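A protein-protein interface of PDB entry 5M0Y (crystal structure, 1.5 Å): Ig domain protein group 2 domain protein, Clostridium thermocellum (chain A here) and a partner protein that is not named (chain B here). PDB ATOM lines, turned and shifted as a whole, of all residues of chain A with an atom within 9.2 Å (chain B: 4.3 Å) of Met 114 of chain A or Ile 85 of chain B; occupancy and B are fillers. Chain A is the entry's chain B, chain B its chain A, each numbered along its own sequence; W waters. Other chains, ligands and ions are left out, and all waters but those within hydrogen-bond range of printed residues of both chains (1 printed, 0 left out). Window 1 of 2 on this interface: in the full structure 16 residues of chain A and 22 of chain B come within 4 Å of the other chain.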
ATOM      1  N   GLY A 100     -26.826  -6.014   6.239  1.00  0.00           N
ATOM      2  CA  GLY A 100     -25.399  -6.001   6.568  1.00  0.00           C
ATOM      3  C   GLY A 100     -24.746  -4.657   6.789  1.00  0.00           C
ATOM      4  O   GLY A 100     -23.524  -4.610   6.860  1.00  0.00           O
ATOM      5  N   VAL A 102     -24.435  -2.944   9.732  1.00  0.00           N
ATOM      6  CA  VAL A 102     -24.760  -3.370  11.081  1.00  0.00           C
ATOM      7  C   VAL A 102     -24.528  -2.234  12.073  1.00  0.00           C
ATOM      8  O   VAL A 102     -23.522  -1.518  11.991  1.00  0.00           O
ATOM      9  CB  VAL A 102     -23.930  -4.621  11.465  1.00  0.00           C
ATOM     10  CG1 VAL A 102     -24.319  -5.130  12.838  1.00  0.00           C
ATOM     11  CG2 VAL A 102     -24.128  -5.735  10.444  1.00  0.00           C
ATOM     12  N   ARG A 104     -23.501  -0.432  15.473  1.00  0.00           N
ATOM     13  CA  ARG A 104     -22.567  -0.533  16.590  1.00  0.00           C
ATOM     14  C   ARG A 104     -22.879   0.625  17.522  1.00  0.00           C
ATOM     15  O   ARG A 104     -22.822   1.782  17.103  1.00  0.00           O
ATOM     16  CB  ARG A 104     -21.125  -0.453  16.096  1.00  0.00           C
ATOM     17  CG  ARG A 104     -20.630  -1.737  15.444  1.00  0.00           C
ATOM     18  CD  ARG A 104     -19.326  -1.492  14.712  1.00  0.00           C
ATOM     19  NE  ARG A 104     -18.684  -2.711  14.213  1.00  0.00           N
ATOM     20  CZ  ARG A 104     -17.720  -3.409  14.826  1.00  0.00           C
ATOM     21  NH1 ARG A 104     -17.248  -3.066  16.025  1.00  0.00           N
ATOM     22  NH2 ARG A 104     -17.216  -4.477  14.222  1.00  0.00           N
ATOM     23  N   ASP A 109     -22.994   3.260   9.598  1.00  0.00           N
ATOM     24  CA  ASP A 109     -22.155   4.181   8.812  1.00  0.00           C
ATOM     25  C   ASP A 109     -22.492   4.235   7.318  1.00  0.00           C
ATOM     26  O   ASP A 109     -21.748   4.823   6.532  1.00  0.00           O
ATOM     27  CB  ASP A 109     -20.661   3.907   9.056  1.00  0.00           C
ATOM     28  CG  ASP A 109     -20.212   2.530   8.584  1.00  0.00           C
ATOM     29  OD1 ASP A 109     -21.007   1.774   7.987  1.00  0.00           O
ATOM     30  OD2 ASP A 109     -19.036   2.185   8.824  1.00  0.00           O
ATOM     31  N   ALA A 111     -22.447   2.059   4.926  1.00  0.00           N
ATOM     32  CA  ALA A 111     -21.583   1.282   4.049  1.00  0.00           C
ATOM     33  C   ALA A 111     -21.607  -0.154   4.530  1.00  0.00           C
ATOM     34  O   ALA A 111     -21.718  -0.392   5.729  1.00  0.00           O
ATOM     35  CB  ALA A 111     -20.153   1.812   4.086  1.00  0.00           C
ATOM     36  N   ILE A 112     -21.540  -1.108   3.608  1.00  0.00           N
ATOM     37  CA  ILE A 112     -21.395  -2.521   3.979  1.00  0.00           C
ATOM     38  C   ILE A 112     -19.937  -2.884   3.756  1.00  0.00           C
ATOM     39  O   ILE A 112     -19.458  -2.808   2.639  1.00  0.00           O
ATOM     40  CB  ILE A 112     -22.301  -3.432   3.134  1.00  0.00           C
ATOM     41  CG1 ILE A 112     -23.774  -3.052   3.379  1.00  0.00           C
ATOM     42  CG2 ILE A 112     -22.031  -4.898   3.460  1.00  0.00           C
ATOM     43  CD1 ILE A 112     -24.790  -3.897   2.631  1.00  0.00           C
ATOM     44  N   ASN A 113     -19.221  -3.280   4.807  1.00  0.00           N
ATOM     45  CA  ASN A 113     -17.799  -3.611   4.650  1.00  0.00           C
ATOM     46  C   ASN A 113     -17.325  -4.495   5.803  1.00  0.00           C
ATOM     47  O   ASN A 113     -18.147  -5.057   6.529  1.00  0.00           O
ATOM     48  CB  ASN A 113     -16.975  -2.306   4.507  1.00  0.00           C
ATOM     49  CG  ASN A 113     -17.097  -1.394   5.707  1.00  0.00           C
ATOM     50  OD1 ASN A 113     -17.317  -1.844   6.822  1.00  0.00           O
ATOM     51  ND2 ASN A 113     -16.939  -0.090   5.480  1.00  0.00           N
ATOM     52  N   MET A 114     -16.008  -4.605   5.996  1.00  0.00           N
ATOM     53  CA  MET A 114     -15.484  -5.544   6.981  1.00  0.00           C
ATOM     54  C   MET A 114     -15.866  -5.203   8.414  1.00  0.00           C
ATOM     55  O   MET A 114     -15.960  -6.096   9.244  1.00  0.00           O
ATOM     56  CB  MET A 114     -13.967  -5.659   6.857  1.00  0.00           C
ATOM     57  CG  MET A 114     -13.405  -6.945   7.423  1.00  0.00           C
ATOM     58  SD  MET A 114     -14.058  -8.379   6.555  1.00  0.00           S
ATOM     59  CE  MET A 114     -12.984  -9.668   7.198  1.00  0.00           C
ATOM     60  N   VAL A 115     -16.111  -3.928   8.712  1.00  0.00           N
ATOM     61  CA  VAL A 115     -16.571  -3.539  10.048  1.00  0.00           C
ATOM     62  C   VAL A 115     -17.857  -4.304  10.385  1.00  0.00           C
ATOM     63  O   VAL A 115     -18.033  -4.803  11.503  1.00  0.00           O
ATOM     64  CB  VAL A 115     -16.782  -2.004  10.162  1.00  0.00           C
ATOM     65  CG1 VAL A 115     -17.344  -1.632  11.525  1.00  0.00           C
ATOM     66  CG2 VAL A 115     -15.488  -1.249   9.884  1.00  0.00           C
ATOM     67  N   ASP A 116     -18.731  -4.445   9.397  1.00  0.00           N
ATOM     68  CA  ASP A 116     -19.996  -5.169   9.587  1.00  0.00           C
ATOM     69  C   ASP A 116     -19.810  -6.661   9.778  1.00  0.00           C
ATOM     70  O   ASP A 116     -20.431  -7.250  10.653  1.00  0.00           O
ATOM     71  CB  ASP A 116     -20.910  -4.884   8.415  1.00  0.00           C
ATOM     72  CG  ASP A 116     -21.130  -3.396   8.230  1.00  0.00           C
ATOM     73  OD1 ASP A 116     -21.704  -2.764   9.141  1.00  0.00           O
ATOM     74  OD2 ASP A 116     -20.698  -2.840   7.202  1.00  0.00           O
ATOM     75  N   VAL A 117     -18.926  -7.257   8.985  1.00  0.00           N
ATOM     76  CA  VAL A 117     -18.566  -8.666   9.126  1.00  0.00           C
ATOM     77  C   VAL A 117     -18.063  -8.941  10.540  1.00  0.00           C
ATOM     78  O   VAL A 117     -18.459  -9.928  11.170  1.00  0.00           O
ATOM     79  CB  VAL A 117     -17.488  -9.073   8.095  1.00  0.00           C
ATOM     80  CG1 VAL A 117     -16.916 -10.460   8.396  1.00  0.00           C
ATOM     81  CG2 VAL A 117     -18.047  -9.002   6.675  1.00  0.00           C
ATOM     82  N   MET A 118     -17.200  -8.062  11.046  1.00  0.00           N
ATOM     83  CA  MET A 118     -16.621  -8.260  12.369  1.00  0.00           C
ATOM     84  C   MET A 118     -17.604  -8.066  13.514  1.00  0.00           C
ATOM     85  O   MET A 118     -17.430  -8.673  14.571  1.00  0.00           O
ATOM     86  CB  MET A 118     -15.382  -7.383  12.553  1.00  0.00           C
ATOM     87  CG  MET A 118     -14.253  -7.726  11.592  1.00  0.00           C
ATOM     88  SD  MET A 118     -13.920  -9.487  11.389  1.00  0.00           S
ATOM     89  CE  MET A 118     -13.225  -9.876  12.985  1.00  0.00           C
ATOM     90  N   GLU A 119     -18.648  -7.270  13.311  1.00  0.00           N
ATOM     91  CA  GLU A 119     -19.694  -7.139  14.326  1.00  0.00           C
ATOM     92  C   GLU A 119     -20.449  -8.465  14.472  1.00  0.00           C
ATOM     93  O   GLU A 119     -20.729  -8.909  15.597  1.00  0.00           O
ATOM     94  CB  GLU A 119     -20.641  -5.991  13.969  1.00  0.00           C
ATOM     95  CG  GLU A 119     -21.755  -5.724  14.968  1.00  0.00           C
ATOM     96  CD  GLU A 119     -21.301  -5.321  16.350  1.00  0.00           C
ATOM     97  OE1 GLU A 119     -20.143  -4.900  16.536  1.00  0.00           O
ATOM     98  OE2 GLU A 119     -22.151  -5.415  17.268  1.00  0.00           O
ATOM     99  N   ILE A 120     -20.762  -9.098  13.346  1.00  0.00           N
ATOM    100  CA  ILE A 120     -21.404 -10.420  13.360  1.00  0.00           C
ATOM    101  C   ILE A 120     -20.458 -11.450  13.976  1.00  0.00           C
ATOM    102  O   ILE A 120     -20.886 -12.310  14.754  1.00  0.00           O
ATOM    103  CB  ILE A 120     -21.862 -10.846  11.948  1.00  0.00           C
ATOM    104  CG1 ILE A 120     -22.963  -9.898  11.459  1.00  0.00           C
ATOM    105  CG2 ILE A 120     -22.384 -12.280  11.940  1.00  0.00           C
ATOM    106  CD1 ILE A 120     -23.244 -10.001   9.986  1.00  0.00           C
ATOM    107  N   SER A 121     -19.174 -11.339  13.655  1.00  0.00           N
ATOM    108  CA  SER A 121     -18.190 -12.287  14.162  1.00  0.00           C
ATOM    109  C   SER A 121     -18.105 -12.319  15.694  1.00  0.00           C
ATOM    110  O   SER A 121     -17.766 -13.350  16.263  1.00  0.00           O
ATOM    111  CB  SER A 121     -16.827 -12.017  13.528  1.00  0.00           C
ATOM    112  OG  SER A 121     -16.893 -12.267  12.133  1.00  0.00           O
ATOM    113  N   LYS A 122     -18.438 -11.209  16.353  1.00  0.00           N
ATOM    114  CA  LYS A 122     -18.460 -11.138  17.835  1.00  0.00           C
ATOM    115  C   LYS A 122     -19.320 -12.227  18.468  1.00  0.00           C
ATOM    116  O   LYS A 122     -19.009 -12.692  19.569  1.00  0.00           O
ATOM    117  CB  LYS A 122     -18.977  -9.787  18.333  1.00  0.00           C
ATOM    118  CG  LYS A 122     -18.076  -8.594  18.080  1.00  0.00           C
ATOM    119  CD  LYS A 122     -18.735  -7.326  18.597  1.00  0.00           C
ATOM    120  CE  LYS A 122     -17.861  -6.110  18.372  1.00  0.00           C
ATOM    121  NZ  LYS A 122     -18.527  -4.866  18.842  1.00  0.00           N
ATOM    122  N   ILE A 150     -22.697 -14.175   7.601  1.00  0.00           N
ATOM    123  CA  ILE A 150     -21.532 -13.456   7.090  1.00  0.00           C
ATOM    124  C   ILE A 150     -21.541 -13.404   5.555  1.00  0.00           C
ATOM    125  O   ILE A 150     -21.238 -12.362   4.968  1.00  0.00           O
ATOM    126  CB  ILE A 150     -20.216 -14.036   7.668  1.00  0.00           C
ATOM    127  CG1 ILE A 150     -20.117 -13.644   9.149  1.00  0.00           C
ATOM    128  CG2 ILE A 150     -18.999 -13.531   6.894  1.00  0.00           C
ATOM    129  CD1 ILE A 150     -19.038 -14.358   9.925  1.00  0.00           C
ATOM    130  N   ALA A 151     -21.912 -14.508   4.904  1.00  0.00           N
ATOM    131  CA  ALA A 151     -21.986 -14.547   3.445  1.00  0.00           C
ATOM    132  C   ALA A 151     -22.999 -13.546   2.871  1.00  0.00           C
ATOM    133  O   ALA A 151     -22.780 -13.010   1.791  1.00  0.00           O
ATOM    134  CB  ALA A 151     -22.307 -15.951   2.959  1.00  0.00           C
ATOM    135  N   VAL A 153     -23.663 -10.573   4.177  1.00  0.00           N
ATOM    136  CA  VAL A 153     -22.956  -9.291   4.218  1.00  0.00           C
ATOM    137  C   VAL A 153     -21.994  -9.184   3.036  1.00  0.00           C
ATOM    138  O   VAL A 153     -21.974  -8.168   2.314  1.00  0.00           O
ATOM    139  CB  VAL A 153     -22.204  -9.094   5.560  1.00  0.00           C
ATOM    140  CG1 VAL A 153     -21.440  -7.779   5.574  1.00  0.00           C
ATOM    141  CG2 VAL A 153     -23.178  -9.146   6.729  1.00  0.00           C
ATOM    142  N   ILE A 154     -21.222 -10.246   2.815  1.00  0.00           N
ATOM    143  CA  ILE A 154     -20.190 -10.249   1.787  1.00  0.00           C
ATOM    144  C   ILE A 154     -20.786 -10.129   0.375  1.00  0.00           C
ATOM    145  O   ILE A 154     -20.174  -9.540  -0.511  1.00  0.00           O
ATOM    146  CB  ILE A 154     -19.253 -11.476   1.930  1.00  0.00           C
ATOM    147  CG1 ILE A 154     -18.498 -11.386   3.269  1.00  0.00           C
ATOM    148  CG2 ILE A 154     -18.259 -11.531   0.775  1.00  0.00           C
ATOM    149  CD1 ILE A 154     -17.809 -12.658   3.713  1.00  0.00           C
ATOM    150  N   ARG A 155     -21.993 -10.652   0.168  1.00  0.00           N
ATOM    151  CA  ARG A 155     -22.654 -10.525  -1.128  1.00  0.00           C
ATOM    152  C   ARG A 155     -22.708  -9.074  -1.626  1.00  0.00           C
ATOM    153  O   ARG A 155     -22.578  -8.836  -2.827  1.00  0.00           O
ATOM    154  CB  ARG A 155     -24.060 -11.115  -1.085  1.00  0.00           C
ATOM    155  CG  ARG A 155     -24.738 -11.144  -2.441  1.00  0.00           C
ATOM    156  CD  ARG A 155     -26.056 -11.888  -2.387  1.00  0.00           C
ATOM    157  NE  ARG A 155     -26.883 -11.571  -3.549  1.00  0.00           N
ATOM    158  CZ  ARG A 155     -28.099 -12.061  -3.770  1.00  0.00           C
ATOM    159  NH1 ARG A 155     -28.652 -12.919  -2.914  1.00  0.00           N
ATOM    160  NH2 ARG A 155     -28.763 -11.698  -4.861  1.00  0.00           N
ATOM    161  N   HIS A 156     -22.888  -8.125  -0.710  1.00  0.00           N
ATOM    162  CA  HIS A 156     -22.911  -6.696  -1.056  1.00  0.00           C
ATOM    163  C   HIS A 156     -21.761  -5.922  -0.414  1.00  0.00           C
ATOM    164  O   HIS A 156     -21.899  -4.767  -0.013  1.00  0.00           O
ATOM    165  CB  HIS A 156     -24.280  -6.106  -0.726  1.00  0.00           C
ATOM    166  CG  HIS A 156     -25.367  -6.674  -1.579  1.00  0.00           C
ATOM    167  ND1 HIS A 156     -25.417  -6.470  -2.940  1.00  0.00           N
ATOM    168  CD2 HIS A 156     -26.407  -7.487  -1.280  1.00  0.00           C
ATOM    169  CE1 HIS A 156     -26.456  -7.115  -3.440  1.00  0.00           C
ATOM    170  NE2 HIS A 156     -27.072  -7.740  -2.453  1.00  0.00           N
ATOM    171  N   PHE A 157     -20.603  -6.570  -0.382  1.00  0.00           N
ATOM    172  CA  PHE A 157     -19.396  -5.963   0.189  1.00  0.00           C
ATOM    173  C   PHE A 157     -19.049  -4.663  -0.536  1.00  0.00           C
ATOM    174  O   PHE A 157     -19.129  -4.572  -1.769  1.00  0.00           O
ATOM    175  CB  PHE A 157     -18.235  -6.952   0.100  1.00  0.00           C
ATOM    176  CG  PHE A 157     -17.129  -6.707   1.090  1.00  0.00           C
ATOM    177  CD1 PHE A 157     -17.319  -6.973   2.442  1.00  0.00           C
ATOM    178  CD2 PHE A 157     -15.884  -6.263   0.656  1.00  0.00           C
ATOM    179  CE1 PHE A 157     -16.291  -6.790   3.355  1.00  0.00           C
ATOM    180  CE2 PHE A 157     -14.858  -6.067   1.564  1.00  0.00           C
ATOM    181  CZ  PHE A 157     -15.065  -6.332   2.909  1.00  0.00           C
ATOM    182  N   ASN A 158     -18.692  -3.657   0.259  1.00  0.00           N
ATOM    183  CA  ASN A 158     -18.377  -2.298  -0.198  1.00  0.00           C
ATOM    184  C   ASN A 158     -19.549  -1.488  -0.762  1.00  0.00           C
ATOM    185  O   ASN A 158     -19.344  -0.397  -1.290  1.00  0.00           O
ATOM    186  CB  ASN A 158     -17.172  -2.297  -1.151  1.00  0.00           C
ATOM    187  CG  ASN A 158     -15.876  -2.647  -0.439  1.00  0.00           C
ATOM    188  OD1 ASN A 158     -15.672  -2.271   0.720  1.00  0.00           O
ATOM    189  ND2 ASN A 158     -14.997  -3.341  -1.131  1.00  0.00           N
ATOM    190  N   ALA A 159     -20.775  -1.972  -0.584  1.00  0.00           N
ATOM    191  CA  ALA A 159     -21.956  -1.257  -1.077  1.00  0.00           C
ATOM    192  C   ALA A 159     -22.207   0.031  -0.299  1.00  0.00           C
ATOM    193  O   ALA A 159     -21.995   0.095   0.908  1.00  0.00           O
ATOM    194  CB  ALA A 159     -23.187  -2.147  -1.001  1.00  0.00           C
ATOM    195  N   PHE B  41      -8.506  -7.617   8.859  1.00  0.00           N
ATOM    196  CA  PHE B  41      -8.260  -6.354   8.187  1.00  0.00           C
ATOM    197  C   PHE B  41      -9.118  -6.207   6.947  1.00  0.00           C
ATOM    198  O   PHE B  41      -9.625  -7.193   6.420  1.00  0.00           O
ATOM    199  CB  PHE B  41      -6.796  -6.264   7.763  1.00  0.00           C
ATOM    200  CG  PHE B  41      -6.425  -7.219   6.667  1.00  0.00           C
ATOM    201  CD1 PHE B  41      -5.987  -8.504   6.959  1.00  0.00           C
ATOM    202  CD2 PHE B  41      -6.523  -6.832   5.332  1.00  0.00           C
ATOM    203  CE1 PHE B  41      -5.647  -9.383   5.943  1.00  0.00           C
ATOM    204  CE2 PHE B  41      -6.187  -7.713   4.311  1.00  0.00           C
ATOM    205  CZ  PHE B  41      -5.746  -8.985   4.615  1.00  0.00           C
ATOM    206  N   GLN B  42      -9.228  -4.967   6.491  1.00  0.00           N
ATOM    207  CA  GLN B  42      -9.623  -4.649   5.123  1.00  0.00           C
ATOM    208  C   GLN B  42      -8.683  -3.552   4.663  1.00  0.00           C
ATOM    209  O   GLN B  42      -8.398  -2.634   5.431  1.00  0.00           O
ATOM    210  CB  GLN B  42     -11.069  -4.160   5.042  1.00  0.00           C
ATOM    211  CG  GLN B  42     -11.491  -3.757   3.629  1.00  0.00           C
ATOM    212  CD  GLN B  42     -12.962  -3.405   3.492  1.00  0.00           C
ATOM    213  OE1 GLN B  42     -13.696  -3.293   4.475  1.00  0.00           O
ATOM    214  NE2 GLN B  42     -13.403  -3.217   2.249  1.00  0.00           N
ATOM    215  N   PHE B  68      -7.998 -12.956  -4.333  1.00  0.00           N
ATOM    216  CA  PHE B  68      -7.422 -12.710  -3.017  1.00  0.00           C
ATOM    217  C   PHE B  68      -5.904 -12.915  -3.038  1.00  0.00           C
ATOM    218  O   PHE B  68      -5.430 -13.986  -3.439  1.00  0.00           O
ATOM    219  CB  PHE B  68      -8.044 -13.582  -1.927  1.00  0.00           C
ATOM    220  CG  PHE B  68      -7.676 -13.108  -0.557  1.00  0.00           C
ATOM    221  CD1 PHE B  68      -8.370 -12.061   0.018  1.00  0.00           C
ATOM    222  CD2 PHE B  68      -6.569 -13.623   0.102  1.00  0.00           C
ATOM    223  CE1 PHE B  68      -7.999 -11.565   1.253  1.00  0.00           C
ATOM    224  CE2 PHE B  68      -6.190 -13.132   1.339  1.00  0.00           C
ATOM    225  CZ  PHE B  68      -6.903 -12.098   1.911  1.00  0.00           C
ATOM    226  N   ILE B  83     -11.743 -16.112   6.890  1.00  0.00           N
ATOM    227  CA  ILE B  83     -12.613 -15.803   5.751  1.00  0.00           C
ATOM    228  C   ILE B  83     -11.936 -14.762   4.866  1.00  0.00           C
ATOM    229  O   ILE B  83     -11.592 -13.688   5.351  1.00  0.00           O
ATOM    230  CB  ILE B  83     -13.949 -15.192   6.210  1.00  0.00           C
ATOM    231  CG1 ILE B  83     -14.695 -16.128   7.148  1.00  0.00           C
ATOM    232  CG2 ILE B  83     -14.845 -14.888   5.015  1.00  0.00           C
ATOM    233  CD1 ILE B  83     -16.130 -15.700   7.318  1.00  0.00           C
ATOM    234  N   GLN B  84     -11.777 -15.073   3.579  1.00  0.00           N
ATOM    235  CA  GLN B  84     -11.197 -14.166   2.583  1.00  0.00           C
ATOM    236  C   GLN B  84     -12.301 -13.469   1.809  1.00  0.00           C
ATOM    237  O   GLN B  84     -13.324 -14.083   1.478  1.00  0.00           O
ATOM    238  CB  GLN B  84     -10.361 -14.941   1.561  1.00  0.00           C
ATOM    239  CG  GLN B  84      -9.156 -15.685   2.101  1.00  0.00           C
ATOM    240  CD  GLN B  84      -8.557 -16.630   1.067  1.00  0.00           C
ATOM    241  OE1 GLN B  84      -9.156 -16.892   0.014  1.00  0.00           O
ATOM    242  NE2 GLN B  84      -7.372 -17.129   1.355  1.00  0.00           N
ATOM    243  N   ILE B  85     -12.090 -12.188   1.510  1.00  0.00           N
ATOM    244  CA  ILE B  85     -13.001 -11.398   0.689  1.00  0.00           C
ATOM    245  C   ILE B  85     -12.151 -10.585  -0.286  1.00  0.00           C
ATOM    246  O   ILE B  85     -11.216  -9.893   0.129  1.00  0.00           O
ATOM    247  CB  ILE B  85     -13.867 -10.428   1.526  1.00  0.00           C
ATOM    248  CG1 ILE B  85     -14.654 -11.183   2.610  1.00  0.00           C
ATOM    249  CG2 ILE B  85     -14.833  -9.661   0.625  1.00  0.00           C
ATOM    250  CD1 ILE B  85     -14.982 -10.344   3.819  1.00  0.00           C
ATOM    251  N   ALA B  86     -12.477 -10.664  -1.575  1.00  0.00           N
ATOM    252  CA  ALA B  86     -11.818  -9.845  -2.591  1.00  0.00           C
ATOM    253  C   ALA B  86     -12.855  -9.042  -3.355  1.00  0.00           C
ATOM    254  O   ALA B  86     -13.881  -9.584  -3.785  1.00  0.00           O
ATOM    255  CB  ALA B  86     -11.016 -10.715  -3.541  1.00  0.00           C
ATOM    256  N   PHE B  97      -9.427  -5.759  -0.497  1.00  0.00           N
ATOM    257  CA  PHE B  97      -9.568  -7.118  -0.008  1.00  0.00           C
ATOM    258  C   PHE B  97      -9.496  -7.129   1.504  1.00  0.00           C
ATOM    259  O   PHE B  97      -9.049  -6.164   2.133  1.00  0.00           O
ATOM    260  CB  PHE B  97      -8.515  -8.046  -0.638  1.00  0.00           C
ATOM    261  CG  PHE B  97      -7.102  -7.567  -0.472  1.00  0.00           C
ATOM    262  CD1 PHE B  97      -6.344  -7.971   0.618  1.00  0.00           C
ATOM    263  CD2 PHE B  97      -6.518  -6.728  -1.411  1.00  0.00           C
ATOM    264  CE1 PHE B  97      -5.042  -7.520   0.783  1.00  0.00           C
ATOM    265  CE2 PHE B  97      -5.218  -6.272  -1.252  1.00  0.00           C
ATOM    266  CZ  PHE B  97      -4.476  -6.677  -0.158  1.00  0.00           C
ATOM    267  N   ALA B  98      -9.980  -8.224   2.074  1.00  0.00           N
ATOM    268  CA  ALA B  98     -10.156  -8.326   3.519  1.00  0.00           C
ATOM    269  C   ALA B  98     -10.073  -9.768   3.953  1.00  0.00           C
ATOM    270  O   ALA B  98     -10.410 -10.674   3.192  1.00  0.00           O
ATOM    271  CB  ALA B  98     -11.499  -7.740   3.925  1.00  0.00           C
ATOM    272  N   LEU B  99      -9.629  -9.970   5.183  1.00  0.00           N
ATOM    273  CA  LEU B  99      -9.514 -11.294   5.751  1.00  0.00           C
ATOM    274  C   LEU B  99      -9.560 -11.173   7.248  1.00  0.00           C
ATOM    275  O   LEU B  99      -8.972 -10.254   7.812  1.00  0.00           O
ATOM    276  CB  LEU B  99      -8.210 -11.948   5.301  1.00  0.00           C
ATOM    277  CG  LEU B  99      -7.647 -13.149   6.065  1.00  0.00           C
ATOM    278  CD1 LEU B  99      -8.541 -14.367   5.927  1.00  0.00           C
ATOM    279  CD2 LEU B  99      -6.236 -13.454   5.577  1.00  0.00           C
ATOM    280  N   ALA B 100     -10.264 -12.091   7.892  1.00  0.00           N
ATOM    281  CA  ALA B 100     -10.300 -12.126   9.345  1.00  0.00           C
ATOM    282  C   ALA B 100     -10.624 -13.516   9.811  1.00  0.00           C
ATOM    283  O   ALA B 100     -11.186 -14.322   9.058  1.00  0.00           O
ATOM    284  CB  ALA B 100     -11.364 -11.173   9.862  1.00  0.00           C
ATOM    285  N   PHE B 152      -8.726  -4.964  12.803  1.00  0.00           N
ATOM    286  CA  PHE B 152      -9.650  -5.445  13.825  1.00  0.00           C
ATOM    287  C   PHE B 152      -8.938  -6.316  14.823  1.00  0.00           C
ATOM    288  O   PHE B 152      -8.010  -7.053  14.472  1.00  0.00           O
ATOM    289  CB  PHE B 152     -10.767  -6.245  13.169  1.00  0.00           C
ATOM    290  CG  PHE B 152     -11.520  -5.459  12.153  1.00  0.00           C
ATOM    291  CD1 PHE B 152     -12.541  -4.610  12.545  1.00  0.00           C
ATOM    292  CD2 PHE B 152     -11.180  -5.529  10.809  1.00  0.00           C
ATOM    293  CE1 PHE B 152     -13.225  -3.850  11.618  1.00  0.00           C
ATOM    294  CE2 PHE B 152     -11.859  -4.771   9.870  1.00  0.00           C
ATOM    295  CZ  PHE B 152     -12.887  -3.938  10.276  1.00  0.00           C
HETATM  296  O   HOH W   1     -13.598  -2.257   7.030  1.00  0.00           O
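The side-chain amide oxygen (OE1) of Gln 42 of chain B is in hydrogen-bond range of the backbone NH (N) of Met 114 of chain A (3.1 Å). NE2 of Gln 42 of chain B lies within hydrogen-bond range of OD1 of Asn 158 of chain A, 2.9 Å away.
Val 102 of chain A touches none of the printed residues of chain B. Printed residues of chain B within 4 Å of Met 114 of chain A: Phe 41 (3.9 Å), Gln 42 (3.1 Å), Ile 85 (3.5 Å), Ala 98 (3.7 Å), Leu 99 (3.7 Å), Ala 100 (3.5 Å) and Phe 152 (3.6 Å). Printed residues of chain B within 4 Å of Val 115 of chain A: Phe 152. Of the printed residues of chain B, Met 118 of chain A touches Ala 100 (3.4 Å) and Phe 152 (3.6 Å). Of the printed residues of chain B, Asn 158 of chain A touches Gln 42 (2.9 Å). Phe 68 of chain B touches none of the printed residues of chain A. Ile 85 of chain B touches just these residues of chain A: Met 114 (3.5 Å), Ile 154 (3.7 Å) and Phe 157 (3.6 Å). No residue of chain A comes within 4 Å of Ala 86 of chain B. Of the printed residues of chain A, Ala 98 of chain B touches Met 114 and Phe 157. The nearest printed residue of chain B that does not touch Met 114 of chain A is Ile 83 of chain B (4.6 Å). The nearest residue of chain A that does not touch Ile 85 of chain B is Val 117 of chain A (4.4 Å). The nearest printed residue of chain A that does not touch Ala 100 of chain B is Val 117 of chain A (5.8 Å).
Water W1 lies within hydrogen-bond range of OE1 of Gln 42 of chain B and N of Val 115 of chain A.
Among the printed residues, pairs that only touch across the chains: Phe 157 of chain A with Gln 42 of chain B, Met 118 of chain A with Ala 100 of chain B, Asn 113 of chain A with Gln 42 of chain B, Met 114 of chain A with Ala 100 of chain B, Met 114 of chain A with Ile 85 of chain B, Phe 157 of chain A with Ile 85 of chain B, Val 115 of chain A with Phe 152 of chain B, Met 118 of chain A with Phe 152 of chain B, Met 114 of chain A with Phe 152 of chain B, Ile 150 of chain A with Ile 83 of chain B, Ile 154 of chain A with Ile 85 of chain B, Met 114 of chain A with Ala 98 of chain B, Met 114 of chain A with Leu 99 of chain B, Met 114 of chain A with Phe 41 of chain B, Ile 154 of chain A with Ile 83 of chain B and Phe 157 of chain A with Ala 98 of chain B.
The guanidinium group (NH2) of Arg 104 of chain A lies within hydrogen-bond range of the backbone carbonyl oxygen (O) of Val 115 of chain A (2.9 Å). O of Ile 112 of chain A lies within hydrogen-bond range of N of Asn 158 of chain A (2.6 Å). N of Asn 113 of chain A lies close to OD2 of Asp 116 of chain A. O of Leu 99 of chain B lies within hydrogen-bond range of N of Phe 41 of chain B (2.9 Å). N of Ile 83 of chain B lies within hydrogen-bond range of O of Ala 100 of chain B (2.9 Å). N of Ile 85 of chain B sits at hydrogen-bond distance from O of Ala 98 of chain B, at 2.8 Å.
Of the 12 printed residues of chain B, 8 touch a printed residue of chain A. Printed residues of chain B that touch a printed residue of chain A: Phe 41, Gln 42, Ile 83, Ile 85, Ala 98, Leu 99, Ala 100 and Phe 152. Printed residues of chain A that touch a printed residue of chain B: Asn 113, Met 114, Val 115, Met 118, Ile 150, Ile 154, Phe 157 and Asn 158. Hydrophobic or aromatic side chains of chain A that line the printed part of chain B: Met 114, Val 115, Met 118, Ile 150, Ile 154 and Phe 157. Among the printed residues, no Asp or Glu carboxylate lies within 4 Å of a Lys or Arg side-chain nitrogen of the other chain.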
